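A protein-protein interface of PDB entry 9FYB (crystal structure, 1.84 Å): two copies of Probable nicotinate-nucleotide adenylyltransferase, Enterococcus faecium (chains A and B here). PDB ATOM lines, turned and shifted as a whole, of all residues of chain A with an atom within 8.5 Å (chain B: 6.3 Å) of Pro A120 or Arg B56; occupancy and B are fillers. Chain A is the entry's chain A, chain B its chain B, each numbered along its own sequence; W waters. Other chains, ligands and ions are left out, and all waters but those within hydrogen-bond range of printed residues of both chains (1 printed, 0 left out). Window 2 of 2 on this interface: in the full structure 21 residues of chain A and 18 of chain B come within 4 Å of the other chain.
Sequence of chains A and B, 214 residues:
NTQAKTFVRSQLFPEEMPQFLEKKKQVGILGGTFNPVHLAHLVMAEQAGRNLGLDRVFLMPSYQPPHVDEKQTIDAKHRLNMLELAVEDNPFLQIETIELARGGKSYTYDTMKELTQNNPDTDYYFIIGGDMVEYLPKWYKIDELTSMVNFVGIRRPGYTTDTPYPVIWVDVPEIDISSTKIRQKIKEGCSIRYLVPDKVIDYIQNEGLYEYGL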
ATOM      1  N   GLU A  22      27.777 -31.026  27.909  1.00  0.00           N
ATOM      2  CA  GLU A  22      27.355 -30.698  26.520  1.00  0.00           C
ATOM      3  C   GLU A  22      28.552 -30.326  25.646  1.00  0.00           C
ATOM      4  O   GLU A  22      29.223 -29.335  25.966  1.00  0.00           O
ATOM      5  CB  GLU A  22      26.325 -29.569  26.513  1.00  0.00           C
ATOM      6  CG  GLU A  22      25.623 -29.410  25.174  1.00  0.00           C
ATOM      7  CD  GLU A  22      25.554 -27.995  24.624  1.00  0.00           C
ATOM      8  OE1 GLU A  22      24.929 -27.138  25.276  1.00  0.00           O
ATOM      9  OE2 GLU A  22      26.116 -27.756  23.541  1.00  0.00           O
ATOM     10  N   LYS A  24      29.961 -28.546  22.560  1.00  0.00           N
ATOM     11  CA  LYS A  24      29.653 -27.597  21.507  1.00  0.00           C
ATOM     12  C   LYS A  24      29.970 -28.233  20.159  1.00  0.00           C
ATOM     13  O   LYS A  24      30.924 -29.002  20.029  1.00  0.00           O
ATOM     14  CB  LYS A  24      30.467 -26.311  21.704  1.00  0.00           C
ATOM     15  CG  LYS A  24      29.722 -25.170  22.414  1.00  0.00           C
ATOM     16  CD  LYS A  24      30.654 -24.379  23.325  1.00  0.00           C
ATOM     17  CE  LYS A  24      30.165 -22.952  23.563  1.00  0.00           C
ATOM     18  NZ  LYS A  24      30.258 -22.078  22.343  1.00  0.00           N
ATOM     19  N   LYS A  25      29.157 -27.933  19.157  1.00  0.00           N
ATOM     20  CA  LYS A  25      29.511 -28.319  17.805  1.00  0.00           C
ATOM     21  C   LYS A  25      30.716 -27.499  17.356  1.00  0.00           C
ATOM     22  O   LYS A  25      30.917 -26.365  17.803  1.00  0.00           O
ATOM     23  CB  LYS A  25      28.322 -28.106  16.870  1.00  0.00           C
ATOM     24  CG  LYS A  25      27.226 -29.134  17.120  1.00  0.00           C
ATOM     25  CD  LYS A  25      26.218 -28.562  18.079  1.00  0.00           C
ATOM     26  CE  LYS A  25      25.106 -29.544  18.405  1.00  0.00           C
ATOM     27  NZ  LYS A  25      24.697 -29.424  19.830  1.00  0.00           N
ATOM     28  N   LYS A 113      28.798 -11.991  14.849  1.00  0.00           N
ATOM     29  CA  LYS A 113      27.830 -11.645  15.885  1.00  0.00           C
ATOM     30  C   LYS A 113      26.526 -12.385  15.666  1.00  0.00           C
ATOM     31  O   LYS A 113      26.032 -13.079  16.559  1.00  0.00           O
ATOM     32  CB  LYS A 113      27.563 -10.134  15.935  1.00  0.00           C
ATOM     33  CG  LYS A 113      27.054  -9.671  17.325  1.00  0.00           C
ATOM     34  CD  LYS A 113      27.074  -8.151  17.549  1.00  0.00           C
ATOM     35  CE  LYS A 113      25.837  -7.480  16.946  1.00  0.00           C
ATOM     36  NZ  LYS A 113      25.696  -6.020  17.269  1.00  0.00           N
ATOM     37  N   GLU A 114      25.958 -12.264  14.475  1.00  0.00           N
ATOM     38  CA  GLU A 114      24.646 -12.872  14.269  1.00  0.00           C
ATOM     39  C   GLU A 114      24.711 -14.390  14.377  1.00  0.00           C
ATOM     40  O   GLU A 114      23.822 -15.011  14.981  1.00  0.00           O
ATOM     41  CB  GLU A 114      24.069 -12.432  12.922  1.00  0.00           C
ATOM     42  CG  GLU A 114      22.638 -12.882  12.717  1.00  0.00           C
ATOM     43  CD  GLU A 114      21.839 -11.928  11.852  1.00  0.00           C
ATOM     44  OE1 GLU A 114      20.637 -12.197  11.606  1.00  0.00           O
ATOM     45  OE2 GLU A 114      22.418 -10.913  11.415  1.00  0.00           O
ATOM     46  N   LEU A 115      25.763 -15.015  13.825  1.00  0.00           N
ATOM     47  CA  LEU A 115      25.810 -16.483  13.819  1.00  0.00           C
ATOM     48  C   LEU A 115      26.035 -17.059  15.207  1.00  0.00           C
ATOM     49  O   LEU A 115      25.458 -18.094  15.545  1.00  0.00           O
ATOM     50  CB  LEU A 115      26.875 -17.027  12.857  1.00  0.00           C
ATOM     51  CG  LEU A 115      26.659 -16.829  11.358  1.00  0.00           C
ATOM     52  CD1 LEU A 115      27.898 -17.294  10.591  1.00  0.00           C
ATOM     53  CD2 LEU A 115      25.428 -17.584  10.884  1.00  0.00           C
ATOM     54  N   THR A 116      26.892 -16.445  16.013  1.00  0.00           N
ATOM     55  CA  THR A 116      27.075 -16.984  17.356  1.00  0.00           C
ATOM     56  C   THR A 116      25.824 -16.786  18.198  1.00  0.00           C
ATOM     57  O   THR A 116      25.490 -17.638  19.029  1.00  0.00           O
ATOM     58  CB  THR A 116      28.262 -16.326  18.045  1.00  0.00           C
ATOM     59  OG1 THR A 116      28.076 -14.912  18.011  1.00  0.00           O
ATOM     60  CG2 THR A 116      29.558 -16.688  17.336  1.00  0.00           C
ATOM     61  N   GLN A 117      25.125 -15.668  18.012  1.00  0.00           N
ATOM     62  CA  GLN A 117      23.847 -15.495  18.703  1.00  0.00           C
ATOM     63  C   GLN A 117      22.796 -16.457  18.153  1.00  0.00           C
ATOM     64  O   GLN A 117      21.988 -17.006  18.918  1.00  0.00           O
ATOM     65  CB  GLN A 117      23.387 -14.035  18.602  1.00  0.00           C
ATOM     66  CG  GLN A 117      24.474 -13.059  19.104  1.00  0.00           C
ATOM     67  CD  GLN A 117      24.094 -11.590  19.028  1.00  0.00           C
ATOM     68  OE1 GLN A 117      23.455 -11.142  18.072  1.00  0.00           O
ATOM     69  NE2 GLN A 117      24.554 -10.816  20.012  1.00  0.00           N
ATOM     70  N   ASN A 118      22.806 -16.698  16.835  1.00  0.00           N
ATOM     71  CA  ASN A 118      21.903 -17.704  16.264  1.00  0.00           C
ATOM     72  C   ASN A 118      22.223 -19.102  16.779  1.00  0.00           C
ATOM     73  O   ASN A 118      21.322 -19.941  16.897  1.00  0.00           O
ATOM     74  CB  ASN A 118      21.980 -17.709  14.731  1.00  0.00           C
ATOM     75  CG  ASN A 118      21.181 -16.589  14.081  1.00  0.00           C
ATOM     76  OD1 ASN A 118      20.462 -15.856  14.742  1.00  0.00           O
ATOM     77  ND2 ASN A 118      21.324 -16.451  12.770  1.00  0.00           N
ATOM     78  N   ASN A 119      23.495 -19.384  17.063  1.00  0.00           N
ATOM     79  CA  ASN A 119      23.956 -20.737  17.385  1.00  0.00           C
ATOM     80  C   ASN A 119      24.884 -20.668  18.582  1.00  0.00           C
ATOM     81  O   ASN A 119      26.107 -20.844  18.458  1.00  0.00           O
ATOM     82  CB  ASN A 119      24.667 -21.374  16.195  1.00  0.00           C
ATOM     83  CG  ASN A 119      23.799 -21.391  14.969  1.00  0.00           C
ATOM     84  OD1 ASN A 119      22.900 -22.208  14.873  1.00  0.00           O
ATOM     85  ND2 ASN A 119      24.042 -20.462  14.035  1.00  0.00           N
ATOM     86  N   PRO A 120      24.330 -20.405  19.764  1.00  0.00           N
ATOM     87  CA  PRO A 120      25.173 -20.229  20.948  1.00  0.00           C
ATOM     88  C   PRO A 120      25.868 -21.506  21.364  1.00  0.00           C
ATOM     89  O   PRO A 120      26.860 -21.441  22.102  1.00  0.00           O
ATOM     90  CB  PRO A 120      24.178 -19.738  22.015  1.00  0.00           C
ATOM     91  CG  PRO A 120      22.851 -20.219  21.546  1.00  0.00           C
ATOM     92  CD  PRO A 120      22.890 -20.259  20.064  1.00  0.00           C
ATOM     93  N   ASP A 121      25.424 -22.653  20.864  1.00  0.00           N
ATOM     94  CA  ASP A 121      26.009 -23.947  21.182  1.00  0.00           C
ATOM     95  C   ASP A 121      27.150 -24.320  20.245  1.00  0.00           C
ATOM     96  O   ASP A 121      27.520 -25.499  20.182  1.00  0.00           O
ATOM     97  CB  ASP A 121      24.941 -25.032  21.072  1.00  0.00           C
ATOM     98  CG  ASP A 121      24.435 -25.191  19.641  1.00  0.00           C
ATOM     99  OD1 ASP A 121      24.140 -24.161  18.977  1.00  0.00           O
ATOM    100  OD2 ASP A 121      24.298 -26.355  19.202  1.00  0.00           O
ATOM    101  N   THR A 122      27.671 -23.370  19.470  1.00  0.00           N
ATOM    102  CA  THR A 122      28.619 -23.688  18.414  1.00  0.00           C
ATOM    103  C   THR A 122      29.916 -22.919  18.629  1.00  0.00           C
ATOM    104  O   THR A 122      29.896 -21.701  18.833  1.00  0.00           O
ATOM    105  CB  THR A 122      28.049 -23.357  17.032  1.00  0.00           C
ATOM    106  OG1 THR A 122      26.856 -24.125  16.813  1.00  0.00           O
ATOM    107  CG2 THR A 122      29.093 -23.672  15.935  1.00  0.00           C
ATOM    108  N   ASP A 123      31.031 -23.641  18.581  1.00  0.00           N
ATOM    109  CA  ASP A 123      32.356 -23.046  18.455  1.00  0.00           C
ATOM    110  C   ASP A 123      32.652 -22.867  16.972  1.00  0.00           C
ATOM    111  O   ASP A 123      32.608 -23.833  16.197  1.00  0.00           O
ATOM    112  CB  ASP A 123      33.416 -23.932  19.114  1.00  0.00           C
ATOM    113  CG  ASP A 123      33.382 -23.870  20.648  1.00  0.00           C
ATOM    114  OD1 ASP A 123      33.102 -22.799  21.212  1.00  0.00           O
ATOM    115  OD2 ASP A 123      33.632 -24.904  21.291  1.00  0.00           O
ATOM    116  N   TYR A 124      32.985 -21.636  16.616  1.00  0.00           N
ATOM    117  CA  TYR A 124      33.247 -21.327  15.196  1.00  0.00           C
ATOM    118  C   TYR A 124      34.745 -21.245  14.910  1.00  0.00           C
ATOM    119  O   TYR A 124      35.500 -20.726  15.737  1.00  0.00           O
ATOM    120  CB  TYR A 124      32.549 -20.035  14.783  1.00  0.00           C
ATOM    121  CG  TYR A 124      31.067 -20.161  14.569  1.00  0.00           C
ATOM    122  CD1 TYR A 124      30.561 -20.776  13.439  1.00  0.00           C
ATOM    123  CD2 TYR A 124      30.175 -19.657  15.495  1.00  0.00           C
ATOM    124  CE1 TYR A 124      29.199 -20.881  13.233  1.00  0.00           C
ATOM    125  CE2 TYR A 124      28.810 -19.756  15.307  1.00  0.00           C
ATOM    126  CZ  TYR A 124      28.322 -20.371  14.171  1.00  0.00           C
ATOM    127  OH  TYR A 124      26.972 -20.464  13.988  1.00  0.00           O
ATOM    128  N   LYS B  25      18.900 -29.649  19.365  1.00  0.00           N
ATOM    129  CA  LYS B  25      18.335 -28.325  19.549  1.00  0.00           C
ATOM    130  C   LYS B  25      16.876 -28.332  19.133  1.00  0.00           C
ATOM    131  O   LYS B  25      16.508 -28.923  18.113  1.00  0.00           O
ATOM    132  CB  LYS B  25      19.150 -27.336  18.714  1.00  0.00           C
ATOM    133  CG  LYS B  25      20.374 -26.846  19.465  1.00  0.00           C
ATOM    134  CD  LYS B  25      21.314 -25.973  18.624  1.00  0.00           C
ATOM    135  CE  LYS B  25      21.105 -26.077  17.110  1.00  0.00           C
ATOM    136  NZ  LYS B  25      22.120 -25.241  16.375  1.00  0.00           N
ATOM    137  N   GLN B  26      16.035 -27.692  19.921  1.00  0.00           N
ATOM    138  CA  GLN B  26      14.619 -27.634  19.578  1.00  0.00           C
ATOM    139  C   GLN B  26      14.293 -26.203  19.195  1.00  0.00           C
ATOM    140  O   GLN B  26      14.238 -25.310  20.050  1.00  0.00           O
ATOM    141  CB  GLN B  26      13.748 -28.105  20.731  1.00  0.00           C
ATOM    142  CG  GLN B  26      14.295 -29.303  21.427  1.00  0.00           C
ATOM    143  CD  GLN B  26      13.335 -30.441  21.349  1.00  0.00           C
ATOM    144  OE1 GLN B  26      13.037 -30.970  20.263  1.00  0.00           O
ATOM    145  NE2 GLN B  26      12.720 -30.733  22.476  1.00  0.00           N
ATOM    146  N   VAL B  27      14.048 -25.985  17.919  1.00  0.00           N
ATOM    147  CA  VAL B  27      14.014 -24.638  17.384  1.00  0.00           C
ATOM    148  C   VAL B  27      12.699 -24.445  16.664  1.00  0.00           C
ATOM    149  O   VAL B  27      12.360 -25.231  15.767  1.00  0.00           O
ATOM    150  CB  VAL B  27      15.189 -24.405  16.423  1.00  0.00           C
ATOM    151  CG1 VAL B  27      14.912 -23.206  15.558  1.00  0.00           C
ATOM    152  CG2 VAL B  27      16.519 -24.284  17.230  1.00  0.00           C
ATOM    153  N   GLY B  28      11.962 -23.394  17.044  1.00  0.00           N
ATOM    154  CA  GLY B  28      10.755 -23.049  16.312  1.00  0.00           C
ATOM    155  C   GLY B  28      11.058 -22.239  15.070  1.00  0.00           C
ATOM    156  O   GLY B  28      12.054 -21.519  14.992  1.00  0.00           O
ATOM    157  N   ILE B  29      10.167 -22.354  14.091  1.00  0.00           N
ATOM    158  CA  ILE B  29      10.218 -21.575  12.857  1.00  0.00           C
ATOM    159  C   ILE B  29       8.858 -20.927  12.669  1.00  0.00           C
ATOM    160  O   ILE B  29       7.850 -21.634  12.588  1.00  0.00           O
ATOM    161  CB  ILE B  29      10.513 -22.455  11.626  1.00  0.00           C
ATOM    162  CG1 ILE B  29      11.811 -23.229  11.814  1.00  0.00           C
ATOM    163  CG2 ILE B  29      10.493 -21.606  10.342  1.00  0.00           C
ATOM    164  CD1 ILE B  29      13.005 -22.377  11.700  1.00  0.00           C
ATOM    165  N   GLY B  49       6.917 -20.761  21.312  1.00  0.00           N
ATOM    166  CA  GLY B  49       8.164 -21.401  21.672  1.00  0.00           C
ATOM    167  C   GLY B  49       8.361 -21.537  23.159  1.00  0.00           C
ATOM    168  O   GLY B  49       8.802 -22.598  23.619  1.00  0.00           O
ATOM    169  N   LEU B  54      10.700 -24.687  23.792  1.00  0.00           N
ATOM    170  CA  LEU B  54      11.727 -24.750  22.764  1.00  0.00           C
ATOM    171  C   LEU B  54      12.943 -23.928  23.178  1.00  0.00           C
ATOM    172  O   LEU B  54      12.881 -23.081  24.075  1.00  0.00           O
ATOM    173  CB  LEU B  54      11.194 -24.258  21.419  1.00  0.00           C
ATOM    174  CG  LEU B  54       9.850 -24.827  20.970  1.00  0.00           C
ATOM    175  CD1 LEU B  54       9.496 -24.295  19.593  1.00  0.00           C
ATOM    176  CD2 LEU B  54       9.877 -26.369  20.965  1.00  0.00           C
ATOM    177  N   ASP B  55      14.067 -24.201  22.510  1.00  0.00           N
ATOM    178  CA  ASP B  55      15.304 -23.479  22.784  1.00  0.00           C
ATOM    179  C   ASP B  55      15.333 -22.099  22.138  1.00  0.00           C
ATOM    180  O   ASP B  55      15.978 -21.186  22.662  1.00  0.00           O
ATOM    181  CB  ASP B  55      16.503 -24.301  22.293  1.00  0.00           C
ATOM    182  CG  ASP B  55      16.706 -25.596  23.091  1.00  0.00           C
ATOM    183  OD1 ASP B  55      16.872 -25.518  24.320  1.00  0.00           O
ATOM    184  OD2 ASP B  55      16.730 -26.690  22.489  1.00  0.00           O
ATOM    185  N   ARG B  56      14.692 -21.989  20.976  1.00  0.00           N
ATOM    186  CA  ARG B  56      14.716 -20.711  20.230  1.00  0.00           C
ATOM    187  C   ARG B  56      13.670 -20.733  19.123  1.00  0.00           C
ATOM    188  O   ARG B  56      13.083 -21.800  18.904  1.00  0.00           O
ATOM    189  CB  ARG B  56      16.080 -20.490  19.571  1.00  0.00           C
ATOM    190  CG  ARG B  56      16.668 -19.106  19.789  1.00  0.00           C
ATOM    191  CD  ARG B  56      17.659 -19.158  20.932  1.00  0.00           C
ATOM    192  NE  ARG B  56      18.390 -17.918  21.112  1.00  0.00           N
ATOM    193  CZ  ARG B  56      19.535 -17.633  20.507  1.00  0.00           C
ATOM    194  NH1 ARG B  56      20.061 -18.495  19.656  1.00  0.00           N
ATOM    195  NH2 ARG B  56      20.142 -16.485  20.750  1.00  0.00           N
ATOM    196  N   VAL B  57      13.259 -19.548  18.686  1.00  0.00           N
ATOM    197  CA  VAL B  57      12.326 -19.428  17.568  1.00  0.00           C
ATOM    198  C   VAL B  57      12.904 -18.435  16.573  1.00  0.00           C
ATOM    199  O   VAL B  57      13.356 -17.348  16.961  1.00  0.00           O
ATOM    200  CB  VAL B  57      10.913 -18.998  18.026  1.00  0.00           C
ATOM    201  CG1 VAL B  57       9.959 -18.823  16.808  1.00  0.00           C
ATOM    202  CG2 VAL B  57      10.346 -20.023  19.022  1.00  0.00           C
ATOM    203  N   PHE B  58      12.922 -18.818  15.297  1.00  0.00           N
ATOM    204  CA  PHE B  58      13.382 -17.951  14.217  1.00  0.00           C
ATOM    205  C   PHE B  58      12.164 -17.490  13.441  1.00  0.00           C
ATOM    206  O   PHE B  58      11.301 -18.308  13.103  1.00  0.00           O
ATOM    207  CB  PHE B  58      14.330 -18.678  13.263  1.00  0.00           C
ATOM    208  CG  PHE B  58      15.652 -19.011  13.863  1.00  0.00           C
ATOM    209  CD1 PHE B  58      15.749 -19.952  14.869  1.00  0.00           C
ATOM    210  CD2 PHE B  58      16.803 -18.330  13.458  1.00  0.00           C
ATOM    211  CE1 PHE B  58      16.999 -20.251  15.461  1.00  0.00           C
ATOM    212  CE2 PHE B  58      18.048 -18.641  14.017  1.00  0.00           C
ATOM    213  CZ  PHE B  58      18.139 -19.593  15.022  1.00  0.00           C
ATOM    214  N   ASN B  90      16.078  -9.408  22.208  1.00  0.00           N
ATOM    215  CA  ASN B  90      15.459 -10.633  22.710  1.00  0.00           C
ATOM    216  C   ASN B  90      16.269 -11.804  22.185  1.00  0.00           C
ATOM    217  O   ASN B  90      16.154 -12.175  21.005  1.00  0.00           O
ATOM    218  CB  ASN B  90      13.999 -10.717  22.279  1.00  0.00           C
ATOM    219  CG  ASN B  90      13.277 -11.914  22.861  1.00  0.00           C
ATOM    220  OD1 ASN B  90      13.855 -12.714  23.594  1.00  0.00           O
ATOM    221  ND2 ASN B  90      11.997 -12.041  22.529  1.00  0.00           N
ATOM    222  N   PRO B  91      17.108 -12.410  23.024  1.00  0.00           N
ATOM    223  CA  PRO B  91      17.900 -13.553  22.556  1.00  0.00           C
ATOM    224  C   PRO B  91      17.049 -14.746  22.174  1.00  0.00           C
ATOM    225  O   PRO B  91      17.526 -15.614  21.443  1.00  0.00           O
ATOM    226  CB  PRO B  91      18.807 -13.872  23.758  1.00  0.00           C
ATOM    227  CG  PRO B  91      18.089 -13.322  24.937  1.00  0.00           C
ATOM    228  CD  PRO B  91      17.348 -12.099  24.445  1.00  0.00           C
ATOM    229  N   PHE B  92      15.796 -14.802  22.620  1.00  0.00           N
ATOM    230  CA  PHE B  92      14.957 -15.949  22.297  1.00  0.00           C
ATOM    231  C   PHE B  92      14.495 -15.941  20.850  1.00  0.00           C
ATOM    232  O   PHE B  92      14.215 -17.008  20.297  1.00  0.00           O
ATOM    233  CB  PHE B  92      13.740 -15.989  23.213  1.00  0.00           C
ATOM    234  CG  PHE B  92      12.985 -17.269  23.123  1.00  0.00           C
ATOM    235  CD1 PHE B  92      13.571 -18.458  23.553  1.00  0.00           C
ATOM    236  CD2 PHE B  92      11.713 -17.305  22.573  1.00  0.00           C
ATOM    237  CE1 PHE B  92      12.882 -19.657  23.474  1.00  0.00           C
ATOM    238  CE2 PHE B  92      11.024 -18.516  22.488  1.00  0.00           C
ATOM    239  CZ  PHE B  92      11.628 -19.684  22.921  1.00  0.00           C
ATOM    240  N   LEU B  93      14.353 -14.761  20.234  1.00  0.00           N
ATOM    241  CA  LEU B  93      13.818 -14.634  18.881  1.00  0.00           C
ATOM    242  C   LEU B  93      14.941 -14.216  17.941  1.00  0.00           C
ATOM    243  O   LEU B  93      15.558 -13.169  18.141  1.00  0.00           O
ATOM    244  CB  LEU B  93      12.674 -13.610  18.824  1.00  0.00           C
ATOM    245  CG  LEU B  93      11.426 -13.938  19.639  1.00  0.00           C
ATOM    246  CD1 LEU B  93      10.312 -12.926  19.358  1.00  0.00           C
ATOM    247  CD2 LEU B  93      10.959 -15.371  19.324  1.00  0.00           C
ATOM    248  N   GLN B  94      15.192 -15.013  16.906  1.00  0.00           N
ATOM    249  CA  GLN B  94      16.228 -14.715  15.926  1.00  0.00           C
ATOM    250  C   GLN B  94      15.596 -14.697  14.546  1.00  0.00           C
ATOM    251  O   GLN B  94      14.410 -14.973  14.382  1.00  0.00           O
ATOM    252  CB  GLN B  94      17.368 -15.735  15.995  1.00  0.00           C
ATOM    253  CG  GLN B  94      17.912 -15.893  17.396  1.00  0.00           C
ATOM    254  CD  GLN B  94      18.568 -14.620  17.867  1.00  0.00           C
ATOM    255  OE1 GLN B  94      18.192 -14.050  18.882  1.00  0.00           O
ATOM    256  NE2 GLN B  94      19.531 -14.150  17.115  1.00  0.00           N
HETATM  257  O   HOH W   1      18.909 -13.315  13.940  1.00  0.00           O
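O of Gln A117 is in hydrogen-bond range of NH1 of Arg B56 (2.5 Å).
The guanidinium group (NH1) of Arg B56 sits at hydrogen-bond distance from the backbone carbonyl oxygen (O) of Asn A118 (3.4 Å).
OD1 of Asn A118 is in hydrogen-bond range of NE2 of Gln B94 (3.1 Å).
The side-chain amino group (NZ) of Lys B25 is in hydrogen-bond range of the side-chain amide oxygen (OD1) of Asn A119, 3.5 Å away.
NZ of Lys B25 lies within salt-bridge range of OD1 of Asp A121 (3.5 Å).
NZ of Lys A24 sits at hydrogen-bond distance from O of Pro A120, 3.5 Å away.
The side-chain amino group of Lys A25 is in salt-bridge range of the side-chain carboxylate of Asp A121 (3.2 Å).
The side-chain hydroxyl of Tyr A124 lies within hydrogen-bond range of the side-chain amide nitrogen of Asn A119, at 2.9 Å.
N of Arg B56 lies within hydrogen-bond range of O of Gln B26 (3.5 Å).
The backbone carbonyl oxygen (O) of Arg B56 lies within hydrogen-bond range of the backbone NH (N) of Gly B28, 2.7 Å away.
The backbone carbonyl oxygen of Gly B28 sits at hydrogen-bond distance from the backbone NH of Phe B58, 2.9 Å away.
Of the printed residues of chain B, Pro A120 touches Arg B56 (3.4 Å).
Printed residues of chain A within 4 Å of Arg B56: Gln A117 (2.5 Å), Asn A118 (3.4 Å) and Pro A120 (3.4 Å).
No residue of chain A comes within 4 Å of Gly B28.
Of the printed residues of chain B, Asn A118 touches Arg B56 (3.4 Å), Phe B58 (3.7 Å) and Gln B94 (3.1 Å).
Of the printed residues of chain A, Gln B94 touches Asn A118.
Of the printed residues of chain B, Asn A119 touches Lys B25.
Glu A22 touches none of the printed residues of chain B.
The nearest printed residue of chain A that does not touch Arg B56 is Asn A119 (4.4 Å).
The nearest printed residue of chain B that does not touch Asn A118 is Lys B25 (5.4 Å).
Position printed for both chains: 25.
Of the 7 pairs that touch across the chains among the printed residues, none has its exchanged pair printed and touching as well.
Among the printed residues, pairs that only touch across the chains: Asn A118 with Phe B58 and Pro A120 with Arg B56.
Water W1 lies within hydrogen-bond range of OD1 of Asn A118, OE1 of Glu A114 and NE2 of Gln B94.
Printed residues of chain B that touch a printed residue of chain A: Lys B25, Arg B56, Phe B58 and Gln B94.
Hydrophobic or aromatic side chains of chain B within 4 Å of the printed part of chain A: Phe B58.
Of the 15 printed residues of chain A, 5 touch a printed residue of chain B.
Hydrophobic or aromatic side chains of chain A that line the printed part of chain B: Pro A120.
Among the printed residues, 7 pairs touch across the chains.
Among the printed residues, Asp or Glu carboxylates within 4 Å of a Lys or Arg side-chain nitrogen of the other chain: Asp A121 with Lys B25 (3.5 Å).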
